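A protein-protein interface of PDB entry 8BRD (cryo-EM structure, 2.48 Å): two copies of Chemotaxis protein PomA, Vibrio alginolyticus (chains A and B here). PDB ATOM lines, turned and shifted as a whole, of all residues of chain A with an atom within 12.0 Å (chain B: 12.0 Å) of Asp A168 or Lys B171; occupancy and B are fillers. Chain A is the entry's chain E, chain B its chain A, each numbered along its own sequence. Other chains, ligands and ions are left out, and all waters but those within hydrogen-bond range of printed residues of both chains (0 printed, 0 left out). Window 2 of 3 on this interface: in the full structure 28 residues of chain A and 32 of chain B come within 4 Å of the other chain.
Val A161 touches Met B26. Val A161 touches Ala B178 (O to CB, 3.6 Å). Ala A162 touches Met B26. Leu A164 touches Ala B178 (CB to CB, 3.7 Å). Ser A165 touches Met B26 (CB to CE, 3.9 Å). Ala B178 touches Ser A165.
Asp A168 touches Lys B171, but with the chains exchanged Lys A171 does not touch Asp B168 (23.3 Å).
Of the 18 printed residues of chain B, 5 touch a printed residue of chain A. Hydrophobic or aromatic side chains of chain B within 4 Å of the printed part of chain A: Met B26, Pro B175 and Ala B178. Of the 18 printed residues of chain A, 6 touch a printed residue of chain B. Hydrophobic or aromatic side chains of chain A that line the printed part of chain B: Val A161 and Leu A164. Along chain A the printed residues that touch a printed residue of chain B span positions 161 to 168.
Asp A168 touches just one residue of chain B: Lys B171 (3.2 Å). Lys B171 touches one residue of chain A. Asn A166 touches just one residue of chain B: Met B26 (3.6 Å). No residue of chain B comes within 4 Å of Met A167. No residue of chain A comes within 4 Å of Asp B169. No residue of chain A comes within 4 Å of Pro B170. Ala B172 touches none of the printed residues of chain A. No residue of chain A comes within 4 Å of Ile B173. Printed residues of chain B within 4 Å of Val A161: Met B26 and Ala B178. Printed residues of chain A within 4 Å of Met B26: Val A161 (3.98 Å), Ala A162 (3.9 Å), Ser A165 (3.9 Å) and Asn A166 (3.6 Å). Of the printed residues of chain A, Ala B178 touches Val A161, Leu A164 and Ser A165. Gly B21 touches none of the printed residues of chain A. Gly B22 touches none of the printed residues of chain A. The nearest residue of chain A that does not touch Lys B171 is Met A167 (4.6 Å). The nearest printed residue of chain A that does not touch Met B26 is Met A163 (6.1 Å).
O of Ala A162 lies within hydrogen-bond range of ND2 of Asn A166, at 2.8 Å. The side-chain carboxylate (OD1) of Asp B169 sits close to the backbone NH (N) of Lys B171 (3.2 Å).
The backbone carbonyl oxygen (O) of Leu A164 lies close to the backbone nitrogen (N) of Pro B175 (3.3 Å). The side-chain amino group (NZ) of Lys B171 is in salt-bridge range of the side-chain carboxylate (OD1) of Asp A168, 3.9 Å away. The side-chain sulfur of Met B26 lies close to the side-chain amide nitrogen of Asn A166, 3.8 Å away. The backbone carbonyl oxygen (O) of Leu A164 sits close to the backbone carbonyl oxygen (O) of Gly B174.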
ATOM      1  N   GLY A 159     -26.379 -14.306 -29.787  1.00  0.00           N
ATOM      2  CA  GLY A 159     -24.982 -13.934 -29.879  1.00  0.00           C
ATOM      3  C   GLY A 159     -24.767 -12.436 -29.827  1.00  0.00           C
ATOM      4  O   GLY A 159     -23.790 -11.963 -29.249  1.00  0.00           O
ATOM      5  N   LEU A 160     -25.672 -11.667 -30.433  1.00  0.00           N
ATOM      6  CA  LEU A 160     -25.571 -10.215 -30.371  1.00  0.00           C
ATOM      7  C   LEU A 160     -25.757  -9.707 -28.947  1.00  0.00           C
ATOM      8  O   LEU A 160     -25.025  -8.824 -28.491  1.00  0.00           O
ATOM      9  CB  LEU A 160     -26.596  -9.582 -31.307  1.00  0.00           C
ATOM     10  CG  LEU A 160     -26.059  -9.138 -32.664  1.00  0.00           C
ATOM     11  CD1 LEU A 160     -27.211  -8.788 -33.584  1.00  0.00           C
ATOM     12  CD2 LEU A 160     -25.107  -7.964 -32.504  1.00  0.00           C
ATOM     13  N   VAL A 161     -26.741 -10.253 -28.230  1.00  0.00           N
ATOM     14  CA  VAL A 161     -26.935  -9.867 -26.836  1.00  0.00           C
ATOM     15  C   VAL A 161     -25.697 -10.206 -26.017  1.00  0.00           C
ATOM     16  O   VAL A 161     -25.238  -9.403 -25.195  1.00  0.00           O
ATOM     17  CB  VAL A 161     -28.197 -10.537 -26.263  1.00  0.00           C
ATOM     18  CG1 VAL A 161     -28.299 -10.288 -24.773  1.00  0.00           C
ATOM     19  CG2 VAL A 161     -29.441 -10.028 -26.972  1.00  0.00           C
ATOM     20  N   ALA A 162     -25.126 -11.394 -26.243  1.00  0.00           N
ATOM     21  CA  ALA A 162     -23.954 -11.810 -25.483  1.00  0.00           C
ATOM     22  C   ALA A 162     -22.722 -10.979 -25.821  1.00  0.00           C
ATOM     23  O   ALA A 162     -21.892 -10.724 -24.943  1.00  0.00           O
ATOM     24  CB  ALA A 162     -23.683 -13.294 -25.718  1.00  0.00           C
ATOM     25  N   MET A 163     -22.567 -10.571 -27.082  1.00  0.00           N
ATOM     26  CA  MET A 163     -21.454  -9.709 -27.463  1.00  0.00           C
ATOM     27  C   MET A 163     -21.593  -8.329 -26.840  1.00  0.00           C
ATOM     28  O   MET A 163     -20.655  -7.816 -26.223  1.00  0.00           O
ATOM     29  CB  MET A 163     -21.375  -9.583 -28.985  1.00  0.00           C
ATOM     30  CG  MET A 163     -20.769 -10.762 -29.702  1.00  0.00           C
ATOM     31  SD  MET A 163     -21.188 -10.747 -31.451  1.00  0.00           S
ATOM     32  CE  MET A 163     -19.756  -9.900 -32.101  1.00  0.00           C
ATOM     33  N   LEU A 164     -22.764  -7.712 -26.999  1.00  0.00           N
ATOM     34  CA  LEU A 164     -22.967  -6.370 -26.474  1.00  0.00           C
ATOM     35  C   LEU A 164     -22.868  -6.340 -24.960  1.00  0.00           C
ATOM     36  O   LEU A 164     -22.442  -5.333 -24.386  1.00  0.00           O
ATOM     37  CB  LEU A 164     -24.320  -5.836 -26.938  1.00  0.00           C
ATOM     38  CG  LEU A 164     -24.464  -5.670 -28.449  1.00  0.00           C
ATOM     39  CD1 LEU A 164     -25.922  -5.584 -28.852  1.00  0.00           C
ATOM     40  CD2 LEU A 164     -23.701  -4.445 -28.908  1.00  0.00           C
ATOM     41  N   SER A 165     -23.246  -7.428 -24.293  1.00  0.00           N
ATOM     42  CA  SER A 165     -23.126  -7.480 -22.844  1.00  0.00           C
ATOM     43  C   SER A 165     -21.687  -7.631 -22.374  1.00  0.00           C
ATOM     44  O   SER A 165     -21.397  -7.319 -21.215  1.00  0.00           O
ATOM     45  CB  SER A 165     -23.967  -8.632 -22.296  1.00  0.00           C
ATOM     46  OG  SER A 165     -25.225  -8.695 -22.939  1.00  0.00           O
ATOM     47  N   ASN A 166     -20.782  -8.092 -23.234  1.00  0.00           N
ATOM     48  CA  ASN A 166     -19.432  -8.474 -22.831  1.00  0.00           C
ATOM     49  C   ASN A 166     -18.394  -7.919 -23.795  1.00  0.00           C
ATOM     50  O   ASN A 166     -17.482  -8.625 -24.229  1.00  0.00           O
ATOM     51  CB  ASN A 166     -19.302  -9.992 -22.748  1.00  0.00           C
ATOM     52  CG  ASN A 166     -20.293 -10.612 -21.791  1.00  0.00           C
ATOM     53  OD1 ASN A 166     -20.301 -10.306 -20.599  1.00  0.00           O
ATOM     54  ND2 ASN A 166     -21.147 -11.487 -22.311  1.00  0.00           N
ATOM     55  N   MET A 167     -18.507  -6.639 -24.146  1.00  0.00           N
ATOM     56  CA  MET A 167     -17.532  -6.056 -25.060  1.00  0.00           C
ATOM     57  C   MET A 167     -16.173  -5.826 -24.414  1.00  0.00           C
ATOM     58  O   MET A 167     -15.198  -5.601 -25.137  1.00  0.00           O
ATOM     59  CB  MET A 167     -18.052  -4.737 -25.637  1.00  0.00           C
ATOM     60  CG  MET A 167     -19.431  -4.824 -26.259  1.00  0.00           C
ATOM     61  SD  MET A 167     -19.496  -4.079 -27.899  1.00  0.00           S
ATOM     62  CE  MET A 167     -19.120  -2.373 -27.523  1.00  0.00           C
ATOM     63  N   ASP A 168     -16.079  -5.882 -23.088  1.00  0.00           N
ATOM     64  CA  ASP A 168     -14.796  -5.744 -22.411  1.00  0.00           C
ATOM     65  C   ASP A 168     -14.043  -7.060 -22.287  1.00  0.00           C
ATOM     66  O   ASP A 168     -12.846  -7.051 -21.977  1.00  0.00           O
ATOM     67  CB  ASP A 168     -14.993  -5.144 -21.018  1.00  0.00           C
ATOM     68  CG  ASP A 168     -15.211  -3.647 -21.057  1.00  0.00           C
ATOM     69  OD1 ASP A 168     -14.594  -2.982 -21.913  1.00  0.00           O
ATOM     70  OD2 ASP A 168     -15.999  -3.135 -20.233  1.00  0.00           O
ATOM     71  N   ASP A 169     -14.706  -8.188 -22.518  1.00  0.00           N
ATOM     72  CA  ASP A 169     -14.090  -9.495 -22.335  1.00  0.00           C
ATOM     73  C   ASP A 169     -13.952 -10.208 -23.671  1.00  0.00           C
ATOM     74  O   ASP A 169     -14.957 -10.697 -24.209  1.00  0.00           O
ATOM     75  CB  ASP A 169     -14.917 -10.338 -21.364  1.00  0.00           C
ATOM     76  CG  ASP A 169     -14.179 -11.571 -20.886  1.00  0.00           C
ATOM     77  OD1 ASP A 169     -12.963 -11.678 -21.150  1.00  0.00           O
ATOM     78  OD2 ASP A 169     -14.815 -12.435 -20.246  1.00  0.00           O
ATOM     79  N   PRO A 170     -12.750 -10.283 -24.250  1.00  0.00           N
ATOM     80  CA  PRO A 170     -12.586 -11.056 -25.493  1.00  0.00           C
ATOM     81  C   PRO A 170     -12.932 -12.528 -25.345  1.00  0.00           C
ATOM     82  O   PRO A 170     -13.449 -13.141 -26.289  1.00  0.00           O
ATOM     83  CB  PRO A 170     -11.101 -10.854 -25.827  1.00  0.00           C
ATOM     84  CG  PRO A 170     -10.723  -9.590 -25.135  1.00  0.00           C
ATOM     85  CD  PRO A 170     -11.519  -9.571 -23.873  1.00  0.00           C
ATOM     86  N   LYS A 171     -12.655 -13.113 -24.175  1.00  0.00           N
ATOM     87  CA  LYS A 171     -12.955 -14.521 -23.943  1.00  0.00           C
ATOM     88  C   LYS A 171     -14.443 -14.812 -24.032  1.00  0.00           C
ATOM     89  O   LYS A 171     -14.827 -15.971 -24.224  1.00  0.00           O
ATOM     90  CB  LYS A 171     -12.424 -14.953 -22.575  1.00  0.00           C
ATOM     91  CG  LYS A 171     -10.960 -14.636 -22.342  1.00  0.00           C
ATOM     92  CD  LYS A 171     -10.074 -15.796 -22.757  1.00  0.00           C
ATOM     93  CE  LYS A 171      -9.170 -16.235 -21.620  1.00  0.00           C
ATOM     94  NZ  LYS A 171      -7.858 -16.740 -22.111  1.00  0.00           N
ATOM     95  N   ALA A 172     -15.287 -13.797 -23.872  1.00  0.00           N
ATOM     96  CA  ALA A 172     -16.714 -13.918 -24.124  1.00  0.00           C
ATOM     97  C   ALA A 172     -17.107 -13.423 -25.505  1.00  0.00           C
ATOM     98  O   ALA A 172     -18.101 -13.898 -26.060  1.00  0.00           O
ATOM     99  CB  ALA A 172     -17.508 -13.145 -23.069  1.00  0.00           C
ATOM    100  N   ILE A 173     -16.343 -12.484 -26.066  1.00  0.00           N
ATOM    101  CA  ILE A 173     -16.632 -11.969 -27.399  1.00  0.00           C
ATOM    102  C   ILE A 173     -16.503 -13.071 -28.438  1.00  0.00           C
ATOM    103  O   ILE A 173     -17.350 -13.205 -29.331  1.00  0.00           O
ATOM    104  CB  ILE A 173     -15.708 -10.778 -27.720  1.00  0.00           C
ATOM    105  CG1 ILE A 173     -16.242  -9.503 -27.075  1.00  0.00           C
ATOM    106  CG2 ILE A 173     -15.565 -10.591 -29.222  1.00  0.00           C
ATOM    107  CD1 ILE A 173     -17.577  -9.070 -27.621  1.00  0.00           C
ATOM    108  N   GLY A 174     -15.450 -13.876 -28.339  1.00  0.00           N
ATOM    109  CA  GLY A 174     -15.208 -14.942 -29.284  1.00  0.00           C
ATOM    110  C   GLY A 174     -16.346 -15.936 -29.406  1.00  0.00           C
ATOM    111  O   GLY A 174     -16.938 -16.100 -30.474  1.00  0.00           O
ATOM    112  N   PRO A 175     -16.657 -16.640 -28.315  1.00  0.00           N
ATOM    113  CA  PRO A 175     -17.765 -17.606 -28.357  1.00  0.00           C
ATOM    114  C   PRO A 175     -19.108 -16.996 -28.713  1.00  0.00           C
ATOM    115  O   PRO A 175     -19.912 -17.659 -29.374  1.00  0.00           O
ATOM    116  CB  PRO A 175     -17.772 -18.186 -26.937  1.00  0.00           C
ATOM    117  CG  PRO A 175     -16.390 -18.010 -26.462  1.00  0.00           C
ATOM    118  CD  PRO A 175     -15.906 -16.729 -27.052  1.00  0.00           C
ATOM    119  N   ALA A 176     -19.385 -15.760 -28.291  1.00  0.00           N
ATOM    120  CA  ALA A 176     -20.668 -15.140 -28.604  1.00  0.00           C
ATOM    121  C   ALA A 176     -20.820 -14.913 -30.103  1.00  0.00           C
ATOM    122  O   ALA A 176     -21.863 -15.230 -30.690  1.00  0.00           O
ATOM    123  CB  ALA A 176     -20.813 -13.828 -27.839  1.00  0.00           C
ATOM    124  N   GLY B  21     -21.934 -18.349 -21.457  1.00  0.00           N
ATOM    125  CA  GLY B  21     -20.922 -17.355 -21.787  1.00  0.00           C
ATOM    126  C   GLY B  21     -20.780 -16.280 -20.726  1.00  0.00           C
ATOM    127  O   GLY B  21     -19.668 -15.899 -20.352  1.00  0.00           O
ATOM    128  N   GLY B  22     -21.901 -15.771 -20.239  1.00  0.00           N
ATOM    129  CA  GLY B  22     -21.932 -14.779 -19.187  1.00  0.00           C
ATOM    130  C   GLY B  22     -22.776 -15.219 -18.012  1.00  0.00           C
ATOM    131  O   GLY B  22     -22.665 -16.350 -17.525  1.00  0.00           O
ATOM    132  N   MET B  26     -28.109 -11.635 -18.242  1.00  0.00           N
ATOM    133  CA  MET B  26     -28.042 -10.948 -19.529  1.00  0.00           C
ATOM    134  C   MET B  26     -29.251 -11.273 -20.398  1.00  0.00           C
ATOM    135  O   MET B  26     -29.782 -10.394 -21.084  1.00  0.00           O
ATOM    136  CB  MET B  26     -26.749 -11.311 -20.257  1.00  0.00           C
ATOM    137  CG  MET B  26     -25.492 -11.033 -19.457  1.00  0.00           C
ATOM    138  SD  MET B  26     -24.070 -11.993 -20.012  1.00  0.00           S
ATOM    139  CE  MET B  26     -24.580 -12.456 -21.665  1.00  0.00           C
ATOM    140  N   MET B 163     -32.076   4.801 -24.627  1.00  0.00           N
ATOM    141  CA  MET B 163     -30.625   4.742 -24.482  1.00  0.00           C
ATOM    142  C   MET B 163     -29.953   5.946 -25.129  1.00  0.00           C
ATOM    143  O   MET B 163     -28.974   6.481 -24.603  1.00  0.00           O
ATOM    144  CB  MET B 163     -30.096   3.445 -25.091  1.00  0.00           C
ATOM    145  CG  MET B 163     -28.588   3.391 -25.231  1.00  0.00           C
ATOM    146  SD  MET B 163     -28.025   2.038 -26.272  1.00  0.00           S
ATOM    147  CE  MET B 163     -28.100   2.812 -27.879  1.00  0.00           C
ATOM    148  N   ASN B 166     -30.077   8.822 -22.879  1.00  0.00           N
ATOM    149  CA  ASN B 166     -29.327   8.684 -21.632  1.00  0.00           C
ATOM    150  C   ASN B 166     -27.995   8.025 -21.961  1.00  0.00           C
ATOM    151  O   ASN B 166     -27.940   6.817 -22.209  1.00  0.00           O
ATOM    152  CB  ASN B 166     -30.105   7.866 -20.602  1.00  0.00           C
ATOM    153  CG  ASN B 166     -31.442   8.486 -20.260  1.00  0.00           C
ATOM    154  OD1 ASN B 166     -31.532   9.352 -19.390  1.00  0.00           O
ATOM    155  ND2 ASN B 166     -32.492   8.042 -20.939  1.00  0.00           N
ATOM    156  N   MET B 167     -27.009   8.834 -22.385  1.00  0.00           N
ATOM    157  CA  MET B 167     -25.697   8.312 -22.864  1.00  0.00           C
ATOM    158  C   MET B 167     -24.455   8.920 -22.149  1.00  0.00           C
ATOM    159  O   MET B 167     -23.706   9.928 -22.519  1.00  0.00           O
ATOM    160  CB  MET B 167     -25.632   8.498 -24.374  1.00  0.00           C
ATOM    161  CG  MET B 167     -25.853   7.320 -25.250  1.00  0.00           C
ATOM    162  SD  MET B 167     -25.648   7.972 -26.919  1.00  0.00           S
ATOM    163  CE  MET B 167     -24.070   7.283 -27.403  1.00  0.00           C
ATOM    164  N   ASP B 168     -24.028   8.285 -21.096  1.00  0.00           N
ATOM    165  CA  ASP B 168     -22.858   8.926 -20.462  1.00  0.00           C
ATOM    166  C   ASP B 168     -21.582   8.143 -20.740  1.00  0.00           C
ATOM    167  O   ASP B 168     -20.733   8.673 -21.456  1.00  0.00           O
ATOM    168  CB  ASP B 168     -23.105   9.183 -18.977  1.00  0.00           C
ATOM    169  CG  ASP B 168     -23.690  10.555 -18.703  1.00  0.00           C
ATOM    170  OD1 ASP B 168     -23.130  11.543 -19.218  1.00  0.00           O
ATOM    171  OD2 ASP B 168     -24.670  10.630 -17.947  1.00  0.00           O
ATOM    172  N   ASP B 169     -21.451   6.951 -20.187  1.00  0.00           N
ATOM    173  CA  ASP B 169     -20.201   6.183 -20.309  1.00  0.00           C
ATOM    174  C   ASP B 169     -20.131   5.487 -21.648  1.00  0.00           C
ATOM    175  O   ASP B 169     -21.054   4.873 -22.043  1.00  0.00           O
ATOM    176  CB  ASP B 169     -20.126   5.147 -19.199  1.00  0.00           C
ATOM    177  CG  ASP B 169     -18.788   4.446 -19.065  1.00  0.00           C
ATOM    178  OD1 ASP B 169     -17.884   4.748 -19.856  1.00  0.00           O
ATOM    179  OD2 ASP B 169     -18.659   3.613 -18.148  1.00  0.00           O
ATOM    180  N   PRO B 170     -19.064   5.676 -22.406  1.00  0.00           N
ATOM    181  CA  PRO B 170     -18.925   4.892 -23.582  1.00  0.00           C
ATOM    182  C   PRO B 170     -19.069   3.363 -23.360  1.00  0.00           C
ATOM    183  O   PRO B 170     -19.393   2.771 -24.314  1.00  0.00           O
ATOM    184  CB  PRO B 170     -17.521   5.389 -23.905  1.00  0.00           C
ATOM    185  CG  PRO B 170     -17.481   6.819 -23.526  1.00  0.00           C
ATOM    186  CD  PRO B 170     -18.082   6.721 -22.158  1.00  0.00           C
ATOM    187  N   LYS B 171     -18.886   2.762 -22.151  1.00  0.00           N
ATOM    188  CA  LYS B 171     -18.897   1.334 -21.867  1.00  0.00           C
ATOM    189  C   LYS B 171     -20.272   0.804 -21.483  1.00  0.00           C
ATOM    190  O   LYS B 171     -20.447  -0.416 -21.417  1.00  0.00           O
ATOM    191  CB  LYS B 171     -17.892   1.010 -20.753  1.00  0.00           C
ATOM    192  CG  LYS B 171     -16.432   1.378 -21.056  1.00  0.00           C
ATOM    193  CD  LYS B 171     -15.945   1.029 -22.475  1.00  0.00           C
ATOM    194  CE  LYS B 171     -16.262  -0.407 -22.904  1.00  0.00           C
ATOM    195  NZ  LYS B 171     -16.321  -0.546 -24.386  1.00  0.00           N
ATOM    196  N   ALA B 172     -21.245   1.678 -21.232  1.00  0.00           N
ATOM    197  CA  ALA B 172     -22.599   1.248 -20.911  1.00  0.00           C
ATOM    198  C   ALA B 172     -23.499   1.149 -22.137  1.00  0.00           C
ATOM    199  O   ALA B 172     -24.599   0.585 -22.039  1.00  0.00           O
ATOM    200  CB  ALA B 172     -23.227   2.204 -19.894  1.00  0.00           C
ATOM    201  N   ILE B 173     -23.056   1.668 -23.282  1.00  0.00           N
ATOM    202  CA  ILE B 173     -23.896   1.660 -24.475  1.00  0.00           C
ATOM    203  C   ILE B 173     -24.127   0.234 -24.959  1.00  0.00           C
ATOM    204  O   ILE B 173     -25.221  -0.107 -25.422  1.00  0.00           O
ATOM    205  CB  ILE B 173     -23.283   2.565 -25.565  1.00  0.00           C
ATOM    206  CG1 ILE B 173     -24.357   2.993 -26.561  1.00  0.00           C
ATOM    207  CG2 ILE B 173     -22.119   1.895 -26.274  1.00  0.00           C
ATOM    208  CD1 ILE B 173     -25.104   4.224 -26.135  1.00  0.00           C
ATOM    209  N   GLY B 174     -23.121  -0.631 -24.828  1.00  0.00           N
ATOM    210  CA  GLY B 174     -23.239  -2.015 -25.218  1.00  0.00           C
ATOM    211  C   GLY B 174     -24.254  -2.794 -24.402  1.00  0.00           C
ATOM    212  O   GLY B 174     -25.143  -3.451 -24.953  1.00  0.00           O
ATOM    213  N   PRO B 175     -24.124  -2.763 -23.070  1.00  0.00           N
ATOM    214  CA  PRO B 175     -25.160  -3.389 -22.234  1.00  0.00           C
ATOM    215  C   PRO B 175     -26.541  -2.791 -22.429  1.00  0.00           C
ATOM    216  O   PRO B 175     -27.536  -3.525 -22.394  1.00  0.00           O
ATOM    217  CB  PRO B 175     -24.635  -3.165 -20.811  1.00  0.00           C
ATOM    218  CG  PRO B 175     -23.175  -3.061 -20.968  1.00  0.00           C
ATOM    219  CD  PRO B 175     -22.946  -2.373 -22.276  1.00  0.00           C
ATOM    220  N   ALA B 176     -26.635  -1.473 -22.637  1.00  0.00           N
ATOM    221  CA  ALA B 176     -27.940  -0.867 -22.885  1.00  0.00           C
ATOM    222  C   ALA B 176     -28.555  -1.393 -24.175  1.00  0.00           C
ATOM    223  O   ALA B 176     -29.750  -1.710 -24.219  1.00  0.00           O
ATOM    224  CB  ALA B 176     -27.816   0.653 -22.923  1.00  0.00           C
ATOM    225  N   MET B 177     -27.752  -1.504 -25.236  1.00  0.00           N
ATOM    226  CA  MET B 177     -28.251  -2.062 -26.485  1.00  0.00           C
ATOM    227  C   MET B 177     -28.627  -3.526 -26.339  1.00  0.00           C
ATOM    228  O   MET B 177     -29.605  -3.975 -26.943  1.00  0.00           O
ATOM    229  CB  MET B 177     -27.218  -1.887 -27.596  1.00  0.00           C
ATOM    230  CG  MET B 177     -27.563  -0.775 -28.564  1.00  0.00           C
ATOM    231  SD  MET B 177     -26.241  -0.363 -29.707  1.00  0.00           S
ATOM    232  CE  MET B 177     -24.918   0.040 -28.579  1.00  0.00           C
ATOM    233  N   ALA B 178     -27.863  -4.289 -25.552  1.00  0.00           N
ATOM    234  CA  ALA B 178     -28.211  -5.687 -25.317  1.00  0.00           C
ATOM    235  C   ALA B 178     -29.552  -5.811 -24.602  1.00  0.00           C
ATOM    236  O   ALA B 178     -30.383  -6.650 -24.968  1.00  0.00           O
ATOM    237  CB  ALA B 178     -27.109  -6.374 -24.514  1.00  0.00           C
ATOM    238  N   VAL B 179     -29.784  -4.971 -23.591  1.00  0.00           N
ATOM    239  CA  VAL B 179     -31.059  -5.005 -22.881  1.00  0.00           C
ATOM    240  C   VAL B 179     -32.201  -4.576 -23.794  1.00  0.00           C
ATOM    241  O   VAL B 179     -33.299  -5.141 -23.731  1.00  0.00           O
ATOM    242  CB  VAL B 179     -30.988  -4.139 -21.609  1.00  0.00           C
ATOM    243  CG1 VAL B 179     -32.341  -4.083 -20.930  1.00  0.00           C
ATOM    244  CG2 VAL B 179     -29.954  -4.696 -20.656  1.00  0.00           C
